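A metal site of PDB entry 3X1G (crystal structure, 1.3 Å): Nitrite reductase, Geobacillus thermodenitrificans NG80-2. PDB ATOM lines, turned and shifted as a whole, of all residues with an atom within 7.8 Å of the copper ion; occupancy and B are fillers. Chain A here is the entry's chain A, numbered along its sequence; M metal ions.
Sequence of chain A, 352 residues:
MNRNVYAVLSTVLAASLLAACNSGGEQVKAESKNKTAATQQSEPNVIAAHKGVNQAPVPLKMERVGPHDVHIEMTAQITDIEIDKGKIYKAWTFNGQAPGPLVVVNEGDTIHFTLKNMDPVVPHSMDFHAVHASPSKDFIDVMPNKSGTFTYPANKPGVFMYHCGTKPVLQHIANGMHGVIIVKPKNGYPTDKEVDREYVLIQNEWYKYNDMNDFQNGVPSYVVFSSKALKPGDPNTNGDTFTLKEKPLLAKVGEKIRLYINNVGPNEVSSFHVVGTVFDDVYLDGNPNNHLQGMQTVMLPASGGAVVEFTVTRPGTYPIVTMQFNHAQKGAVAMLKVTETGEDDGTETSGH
The backbone NH (N) of Ser 125 sits close to the side-chain sulfur (SG) of Cys 164.
NE2 of His 124 is in hydrogen-bond range of OD2 of Asp 119, at 2.8 Å.
SG of Cys 164 sits close to OG1 of Thr 166 (3.5 Å).
A ring nitrogen (NE2) of His 124 lies close to the backbone carbonyl oxygen (O) of Val 122, 3.4 Å away.
The backbone NH (N) of Met 177 sits close to the backbone carbonyl oxygen (O) of Trp 92 (3.3 Å).
Within 4 Å of the copper ion: His 124, Cys 164, His 172 and Met 177.
The copper ion is bound by ND1 of His 172 (2.0 Å).
The copper ion is bound by ND1 of His 124 (2.0 Å).
The side-chain sulfur (SG) of Cys 164 is bound to the copper ion (2.2 Å).
The copper ion is bound by SD of Met 177 (2.6 Å).
The copper ion has four donor atoms within binding distance.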
ATOM      1  N   ALA A  76     -15.089  -4.644  14.719  1.00  0.00           N
ATOM      2  CA  ALA A  76     -16.314  -4.146  14.125  1.00  0.00           C
ATOM      3  C   ALA A  76     -16.492  -2.736  14.647  1.00  0.00           C
ATOM      4  O   ALA A  76     -16.427  -2.512  15.875  1.00  0.00           O
ATOM      5  CB  ALA A  76     -17.510  -5.027  14.523  1.00  0.00           C
ATOM      6  N   TRP A  92     -21.233   0.516   8.767  1.00  0.00           N
ATOM      7  CA  TRP A  92     -20.902  -0.598   9.689  1.00  0.00           C
ATOM      8  C   TRP A  92     -19.761  -1.332   9.034  1.00  0.00           C
ATOM      9  O   TRP A  92     -19.859  -1.714   7.878  1.00  0.00           O
ATOM     10  CB  TRP A  92     -22.087  -1.531   9.888  1.00  0.00           C
ATOM     11  CG  TRP A  92     -23.328  -0.907  10.446  1.00  0.00           C
ATOM     12  CD1 TRP A  92     -23.646   0.403  10.640  1.00  0.00           C
ATOM     13  CD2 TRP A  92     -24.462  -1.661  10.864  1.00  0.00           C
ATOM     14  NE1 TRP A  92     -24.903   0.520  11.201  1.00  0.00           N
ATOM     15  CE2 TRP A  92     -25.443  -0.746  11.320  1.00  0.00           C
ATOM     16  CE3 TRP A  92     -24.775  -3.016  10.841  1.00  0.00           C
ATOM     17  CZ2 TRP A  92     -26.691  -1.173  11.806  1.00  0.00           C
ATOM     18  CZ3 TRP A  92     -26.028  -3.417  11.275  1.00  0.00           C
ATOM     19  CH2 TRP A  92     -26.975  -2.507  11.761  1.00  0.00           C
ATOM     20  N   THR A  93     -18.626  -1.447   9.731  1.00  0.00           N
ATOM     21  CA  THR A  93     -17.415  -1.870   9.089  1.00  0.00           C
ATOM     22  C   THR A  93     -16.609  -2.881   9.934  1.00  0.00           C
ATOM     23  O   THR A  93     -16.780  -2.951  11.173  1.00  0.00           O
ATOM     24  CB  THR A  93     -16.453  -0.670   8.858  1.00  0.00           C
ATOM     25  OG1 THR A  93     -15.821  -0.245  10.076  1.00  0.00           O
ATOM     26  CG2 THR A  93     -17.134   0.487   8.199  1.00  0.00           C
ATOM     27  N   PHE A  94     -15.701  -3.530   9.253  1.00  0.00           N
ATOM     28  CA  PHE A  94     -14.511  -4.094   9.856  1.00  0.00           C
ATOM     29  C   PHE A  94     -13.388  -3.108   9.742  1.00  0.00           C
ATOM     30  O   PHE A  94     -13.018  -2.675   8.649  1.00  0.00           O
ATOM     31  CB  PHE A  94     -14.131  -5.426   9.226  1.00  0.00           C
ATOM     32  CG  PHE A  94     -15.206  -6.491   9.325  1.00  0.00           C
ATOM     33  CD1 PHE A  94     -15.466  -7.106  10.550  1.00  0.00           C
ATOM     34  CD2 PHE A  94     -16.038  -6.813   8.245  1.00  0.00           C
ATOM     35  CE1 PHE A  94     -16.379  -8.134  10.628  1.00  0.00           C
ATOM     36  CE2 PHE A  94     -16.981  -7.841   8.365  1.00  0.00           C
ATOM     37  CZ  PHE A  94     -17.198  -8.449   9.562  1.00  0.00           C
ATOM     38  N   LEU A 115     -12.478 -11.067  16.829  1.00  0.00           N
ATOM     39  CA  LEU A 115     -13.274  -9.916  16.494  1.00  0.00           C
ATOM     40  C   LEU A 115     -13.477  -9.138  17.776  1.00  0.00           C
ATOM     41  O   LEU A 115     -14.045  -9.651  18.744  1.00  0.00           O
ATOM     42  CB  LEU A 115     -14.634 -10.297  15.879  1.00  0.00           C
ATOM     43  CG  LEU A 115     -15.508  -9.127  15.430  1.00  0.00           C
ATOM     44  CD1 LEU A 115     -14.844  -8.338  14.312  1.00  0.00           C
ATOM     45  CD2 LEU A 115     -16.870  -9.658  15.001  1.00  0.00           C
ATOM     46  N   ASN A 117     -15.569  -6.109  19.078  1.00  0.00           N
ATOM     47  CA  ASN A 117     -16.777  -5.346  18.688  1.00  0.00           C
ATOM     48  C   ASN A 117     -16.754  -3.970  19.381  1.00  0.00           C
ATOM     49  O   ASN A 117     -17.003  -3.921  20.596  1.00  0.00           O
ATOM     50  CB  ASN A 117     -18.038  -6.092  18.968  1.00  0.00           C
ATOM     51  CG  ASN A 117     -19.247  -5.417  18.366  1.00  0.00           C
ATOM     52  OD1 ASN A 117     -19.101  -4.335  17.729  1.00  0.00           O
ATOM     53  ND2 ASN A 117     -20.443  -5.926  18.604  1.00  0.00           N
ATOM     54  N   ASP A 119     -18.793  -1.504  18.284  1.00  0.00           N
ATOM     55  CA  ASP A 119     -20.096  -0.917  18.134  1.00  0.00           C
ATOM     56  C   ASP A 119     -20.757  -0.833  19.541  1.00  0.00           C
ATOM     57  O   ASP A 119     -20.750  -1.819  20.249  1.00  0.00           O
ATOM     58  CB  ASP A 119     -20.924  -1.858  17.230  1.00  0.00           C
ATOM     59  CG  ASP A 119     -22.249  -1.278  16.784  1.00  0.00           C
ATOM     60  OD1 ASP A 119     -22.976  -0.622  17.632  1.00  0.00           O
ATOM     61  OD2 ASP A 119     -22.687  -1.447  15.628  1.00  0.00           O
ATOM     62  N   VAL A 122     -24.853  -2.689  18.609  1.00  0.00           N
ATOM     63  CA  VAL A 122     -25.224  -3.832  17.710  1.00  0.00           C
ATOM     64  C   VAL A 122     -24.182  -4.941  17.828  1.00  0.00           C
ATOM     65  O   VAL A 122     -22.980  -4.659  17.681  1.00  0.00           O
ATOM     66  CB  VAL A 122     -25.400  -3.368  16.219  1.00  0.00           C
ATOM     67  CG1 VAL A 122     -26.010  -4.481  15.431  1.00  0.00           C
ATOM     68  CG2 VAL A 122     -26.240  -2.102  16.138  1.00  0.00           C
ATOM     69  N   PRO A 123     -24.626  -6.203  18.004  1.00  0.00           N
ATOM     70  CA  PRO A 123     -23.700  -7.334  17.892  1.00  0.00           C
ATOM     71  C   PRO A 123     -23.167  -7.480  16.430  1.00  0.00           C
ATOM     72  O   PRO A 123     -23.879  -7.098  15.496  1.00  0.00           O
ATOM     73  CB  PRO A 123     -24.524  -8.584  18.287  1.00  0.00           C
ATOM     74  CG  PRO A 123     -25.714  -8.022  18.964  1.00  0.00           C
ATOM     75  CD  PRO A 123     -25.968  -6.655  18.328  1.00  0.00           C
ATOM     76  N   HIS A 124     -22.001  -8.079  16.303  1.00  0.00           N
ATOM     77  CA  HIS A 124     -21.432  -8.373  14.992  1.00  0.00           C
ATOM     78  C   HIS A 124     -20.751  -9.729  15.005  1.00  0.00           C
ATOM     79  O   HIS A 124     -20.468 -10.280  16.084  1.00  0.00           O
ATOM     80  CB  HIS A 124     -20.491  -7.261  14.494  1.00  0.00           C
ATOM     81  CG  HIS A 124     -21.143  -5.964  14.357  1.00  0.00           C
ATOM     82  ND1 HIS A 124     -22.041  -5.686  13.357  1.00  0.00           N
ATOM     83  CD2 HIS A 124     -21.077  -4.823  15.097  1.00  0.00           C
ATOM     84  CE1 HIS A 124     -22.512  -4.462  13.489  1.00  0.00           C
ATOM     85  NE2 HIS A 124     -21.968  -3.938  14.543  1.00  0.00           N
ATOM     86  N   SER A 125     -20.388 -10.246  13.842  1.00  0.00           N
ATOM     87  CA  SER A 125     -19.843 -11.585  13.707  1.00  0.00           C
ATOM     88  C   SER A 125     -19.015 -11.637  12.437  1.00  0.00           C
ATOM     89  O   SER A 125     -18.946 -10.608  11.695  1.00  0.00           O
ATOM     90  CB  SER A 125     -20.918 -12.641  13.655  1.00  0.00           C
ATOM     91  OG  SER A 125     -21.812 -12.385  12.563  1.00  0.00           O
ATOM     92  N   MET A 126     -18.386 -12.770  12.156  1.00  0.00           N
ATOM     93  CA  MET A 126     -17.576 -12.934  10.950  1.00  0.00           C
ATOM     94  C   MET A 126     -17.807 -14.331  10.354  1.00  0.00           C
ATOM     95  O   MET A 126     -17.677 -15.352  11.013  1.00  0.00           O
ATOM     96  CB  MET A 126     -16.064 -12.848  11.298  1.00  0.00           C
ATOM     97  CG  MET A 126     -15.143 -13.086  10.163  1.00  0.00           C
ATOM     98  SD  MET A 126     -15.336 -11.971   8.708  1.00  0.00           S
ATOM     99  CE  MET A 126     -14.285 -10.640   9.285  1.00  0.00           C
ATOM    100  N   ASP A 141     -22.224 -14.364  17.229  1.00  0.00           N
ATOM    101  CA  ASP A 141     -22.131 -12.958  17.567  1.00  0.00           C
ATOM    102  C   ASP A 141     -21.148 -12.657  18.682  1.00  0.00           C
ATOM    103  O   ASP A 141     -21.001 -13.433  19.643  1.00  0.00           O
ATOM    104  CB  ASP A 141     -23.494 -12.411  17.958  1.00  0.00           C
ATOM    105  CG  ASP A 141     -24.468 -12.286  16.805  1.00  0.00           C
ATOM    106  OD1 ASP A 141     -24.059 -12.407  15.587  1.00  0.00           O
ATOM    107  OD2 ASP A 141     -25.699 -12.236  17.044  1.00  0.00           O
ATOM    108  N   HIS A 163     -17.776 -11.633   5.403  1.00  0.00           N
ATOM    109  CA  HIS A 163     -18.791 -10.634   5.770  1.00  0.00           C
ATOM    110  C   HIS A 163     -19.353 -10.943   7.172  1.00  0.00           C
ATOM    111  O   HIS A 163     -19.286 -12.080   7.648  1.00  0.00           O
ATOM    112  CB  HIS A 163     -19.939 -10.625   4.751  1.00  0.00           C
ATOM    113  CG  HIS A 163     -20.719 -11.889   4.766  1.00  0.00           C
ATOM    114  ND1 HIS A 163     -21.797 -12.096   5.603  1.00  0.00           N
ATOM    115  CD2 HIS A 163     -20.547 -13.060   4.119  1.00  0.00           C
ATOM    116  CE1 HIS A 163     -22.246 -13.363   5.481  1.00  0.00           C
ATOM    117  NE2 HIS A 163     -21.492 -13.966   4.594  1.00  0.00           N
ATOM    118  N   CYS A 164     -19.976  -9.939   7.765  1.00  0.00           N
ATOM    119  CA  CYS A 164     -20.721 -10.151   9.033  1.00  0.00           C
ATOM    120  C   CYS A 164     -21.818 -11.134   8.786  1.00  0.00           C
ATOM    121  O   CYS A 164     -22.543 -11.030   7.785  1.00  0.00           O
ATOM    122  CB  CYS A 164     -21.142  -8.788   9.581  1.00  0.00           C
ATOM    123  SG  CYS A 164     -22.064  -8.903  11.070  1.00  0.00           S
ATOM    124  N   GLY A 165     -22.059 -11.999   9.783  1.00  0.00           N
ATOM    125  CA  GLY A 165     -23.097 -13.010   9.746  1.00  0.00           C
ATOM    126  C   GLY A 165     -24.206 -12.854  10.747  1.00  0.00           C
ATOM    127  O   GLY A 165     -24.866 -13.817  11.070  1.00  0.00           O
ATOM    128  N   THR A 166     -24.423 -11.606  11.204  1.00  0.00           N
ATOM    129  CA  THR A 166     -25.424 -11.358  12.246  1.00  0.00           C
ATOM    130  C   THR A 166     -26.750 -11.049  11.615  1.00  0.00           C
ATOM    131  O   THR A 166     -26.848 -10.252  10.686  1.00  0.00           O
ATOM    132  CB  THR A 166     -24.901 -10.177  13.090  1.00  0.00           C
ATOM    133  OG1 THR A 166     -23.650 -10.562  13.728  1.00  0.00           O
ATOM    134  CG2 THR A 166     -25.912  -9.768  14.184  1.00  0.00           C
ATOM    135  N   LYS A 167     -27.809 -11.627  12.159  1.00  0.00           N
ATOM    136  CA  LYS A 167     -29.122 -11.422  11.573  1.00  0.00           C
ATOM    137  C   LYS A 167     -29.596  -9.993  11.901  1.00  0.00           C
ATOM    138  O   LYS A 167     -29.428  -9.501  13.064  1.00  0.00           O
ATOM    139  CB  LYS A 167     -30.133 -12.381  12.225  1.00  0.00           C
ATOM    140  CG  LYS A 167     -31.542 -12.320  11.703  1.00  0.00           C
ATOM    141  CD  LYS A 167     -32.499 -13.305  12.422  1.00  0.00           C
ATOM    142  CE  LYS A 167     -34.003 -13.148  12.019  1.00  0.00           C
ATOM    143  NZ  LYS A 167     -34.951 -14.281  12.347  1.00  0.00           N
ATOM    144  N   PRO A 168     -30.289  -9.298  10.953  1.00  0.00           N
ATOM    145  CA  PRO A 168     -30.459  -9.667   9.550  1.00  0.00           C
ATOM    146  C   PRO A 168     -29.141  -9.473   8.764  1.00  0.00           C
ATOM    147  O   PRO A 168     -28.607  -8.341   8.725  1.00  0.00           O
ATOM    148  CB  PRO A 168     -31.512  -8.718   9.020  1.00  0.00           C
ATOM    149  CG  PRO A 168     -31.971  -7.922  10.189  1.00  0.00           C
ATOM    150  CD  PRO A 168     -30.894  -7.979  11.226  1.00  0.00           C
ATOM    151  N   VAL A 169     -28.659 -10.535   8.142  1.00  0.00           N
ATOM    152  CA  VAL A 169     -27.362 -10.450   7.449  1.00  0.00           C
ATOM    153  C   VAL A 169     -27.389  -9.433   6.335  1.00  0.00           C
ATOM    154  O   VAL A 169     -26.419  -8.704   6.152  1.00  0.00           O
ATOM    155  CB  VAL A 169     -26.960 -11.875   6.981  1.00  0.00           C
ATOM    156  CG1 VAL A 169     -25.710 -11.833   6.108  1.00  0.00           C
ATOM    157  CG2 VAL A 169     -26.722 -12.784   8.180  1.00  0.00           C
ATOM    158  N   GLN A 171     -28.794  -6.596   6.367  1.00  0.00           N
ATOM    159  CA  GLN A 171     -28.534  -5.289   6.972  1.00  0.00           C
ATOM    160  C   GLN A 171     -27.064  -5.079   7.218  1.00  0.00           C
ATOM    161  O   GLN A 171     -26.515  -4.004   6.963  1.00  0.00           O
ATOM    162  CB  GLN A 171     -29.372  -5.135   8.254  1.00  0.00           C
ATOM    163  CG  GLN A 171     -29.264  -3.766   8.874  1.00  0.00           C
ATOM    164  CD  GLN A 171     -30.170  -3.654  10.080  1.00  0.00           C
ATOM    165  OE1 GLN A 171     -30.618  -4.651  10.652  1.00  0.00           O
ATOM    166  NE2 GLN A 171     -30.479  -2.424  10.454  1.00  0.00           N
ATOM    167  N   HIS A 172     -26.406  -6.090   7.805  1.00  0.00           N
ATOM    168  CA  HIS A 172     -25.012  -5.965   8.165  1.00  0.00           C
ATOM    169  C   HIS A 172     -24.118  -5.843   6.914  1.00  0.00           C
ATOM    170  O   HIS A 172     -23.218  -5.013   6.870  1.00  0.00           O
ATOM    171  CB  HIS A 172     -24.572  -7.098   9.073  1.00  0.00           C
ATOM    172  CG  HIS A 172     -25.170  -6.998  10.443  1.00  0.00           C
ATOM    173  ND1 HIS A 172     -24.367  -6.656  11.508  1.00  0.00           N
ATOM    174  CD2 HIS A 172     -26.446  -7.134  10.882  1.00  0.00           C
ATOM    175  CE1 HIS A 172     -25.152  -6.587  12.599  1.00  0.00           C
ATOM    176  NE2 HIS A 172     -26.392  -6.899  12.216  1.00  0.00           N
ATOM    177  N   ILE A 173     -24.404  -6.669   5.881  1.00  0.00           N
ATOM    178  CA  ILE A 173     -23.615  -6.571   4.651  1.00  0.00           C
ATOM    179  C   ILE A 173     -23.878  -5.235   3.996  1.00  0.00           C
ATOM    180  O   ILE A 173     -22.938  -4.515   3.584  1.00  0.00           O
ATOM    181  CB  ILE A 173     -23.894  -7.716   3.685  1.00  0.00           C
ATOM    182  CG1 ILE A 173     -23.548  -9.086   4.298  1.00  0.00           C
ATOM    183  CG2 ILE A 173     -23.104  -7.539   2.396  1.00  0.00           C
ATOM    184  CD1 ILE A 173     -23.885 -10.275   3.421  1.00  0.00           C
ATOM    185  N   ASN A 175     -24.798  -2.377   5.034  1.00  0.00           N
ATOM    186  CA  ASN A 175     -24.226  -1.257   5.735  1.00  0.00           C
ATOM    187  C   ASN A 175     -22.697  -1.206   5.682  1.00  0.00           C
ATOM    188  O   ASN A 175     -22.119  -0.192   6.117  1.00  0.00           O
ATOM    189  CB  ASN A 175     -24.695  -1.186   7.180  1.00  0.00           C
ATOM    190  CG  ASN A 175     -26.089  -0.627   7.317  1.00  0.00           C
ATOM    191  OD1 ASN A 175     -26.526   0.261   6.585  1.00  0.00           O
ATOM    192  ND2 ASN A 175     -26.792  -1.105   8.342  1.00  0.00           N
ATOM    193  N   GLY A 176     -22.037  -2.218   5.133  1.00  0.00           N
ATOM    194  CA  GLY A 176     -20.633  -2.182   4.850  1.00  0.00           C
ATOM    195  C   GLY A 176     -19.774  -3.347   5.325  1.00  0.00           C
ATOM    196  O   GLY A 176     -18.564  -3.305   5.098  1.00  0.00           O
ATOM    197  N   MET A 177     -20.381  -4.365   5.964  1.00  0.00           N
ATOM    198  CA  MET A 177     -19.524  -5.387   6.609  1.00  0.00           C
ATOM    199  C   MET A 177     -19.278  -6.573   5.670  1.00  0.00           C
ATOM    200  O   MET A 177     -19.835  -7.660   5.765  1.00  0.00           O
ATOM    201  CB  MET A 177     -20.229  -5.883   7.894  1.00  0.00           C
ATOM    202  CG  MET A 177     -20.497  -4.726   8.853  1.00  0.00           C
ATOM    203  SD  MET A 177     -20.863  -5.143  10.545  1.00  0.00           S
ATOM    204  CE  MET A 177     -19.262  -5.591  11.150  1.00  0.00           C
HETATM  205 CU    CU M   1     -22.399  -6.871  11.727  1.00  0.00          CU
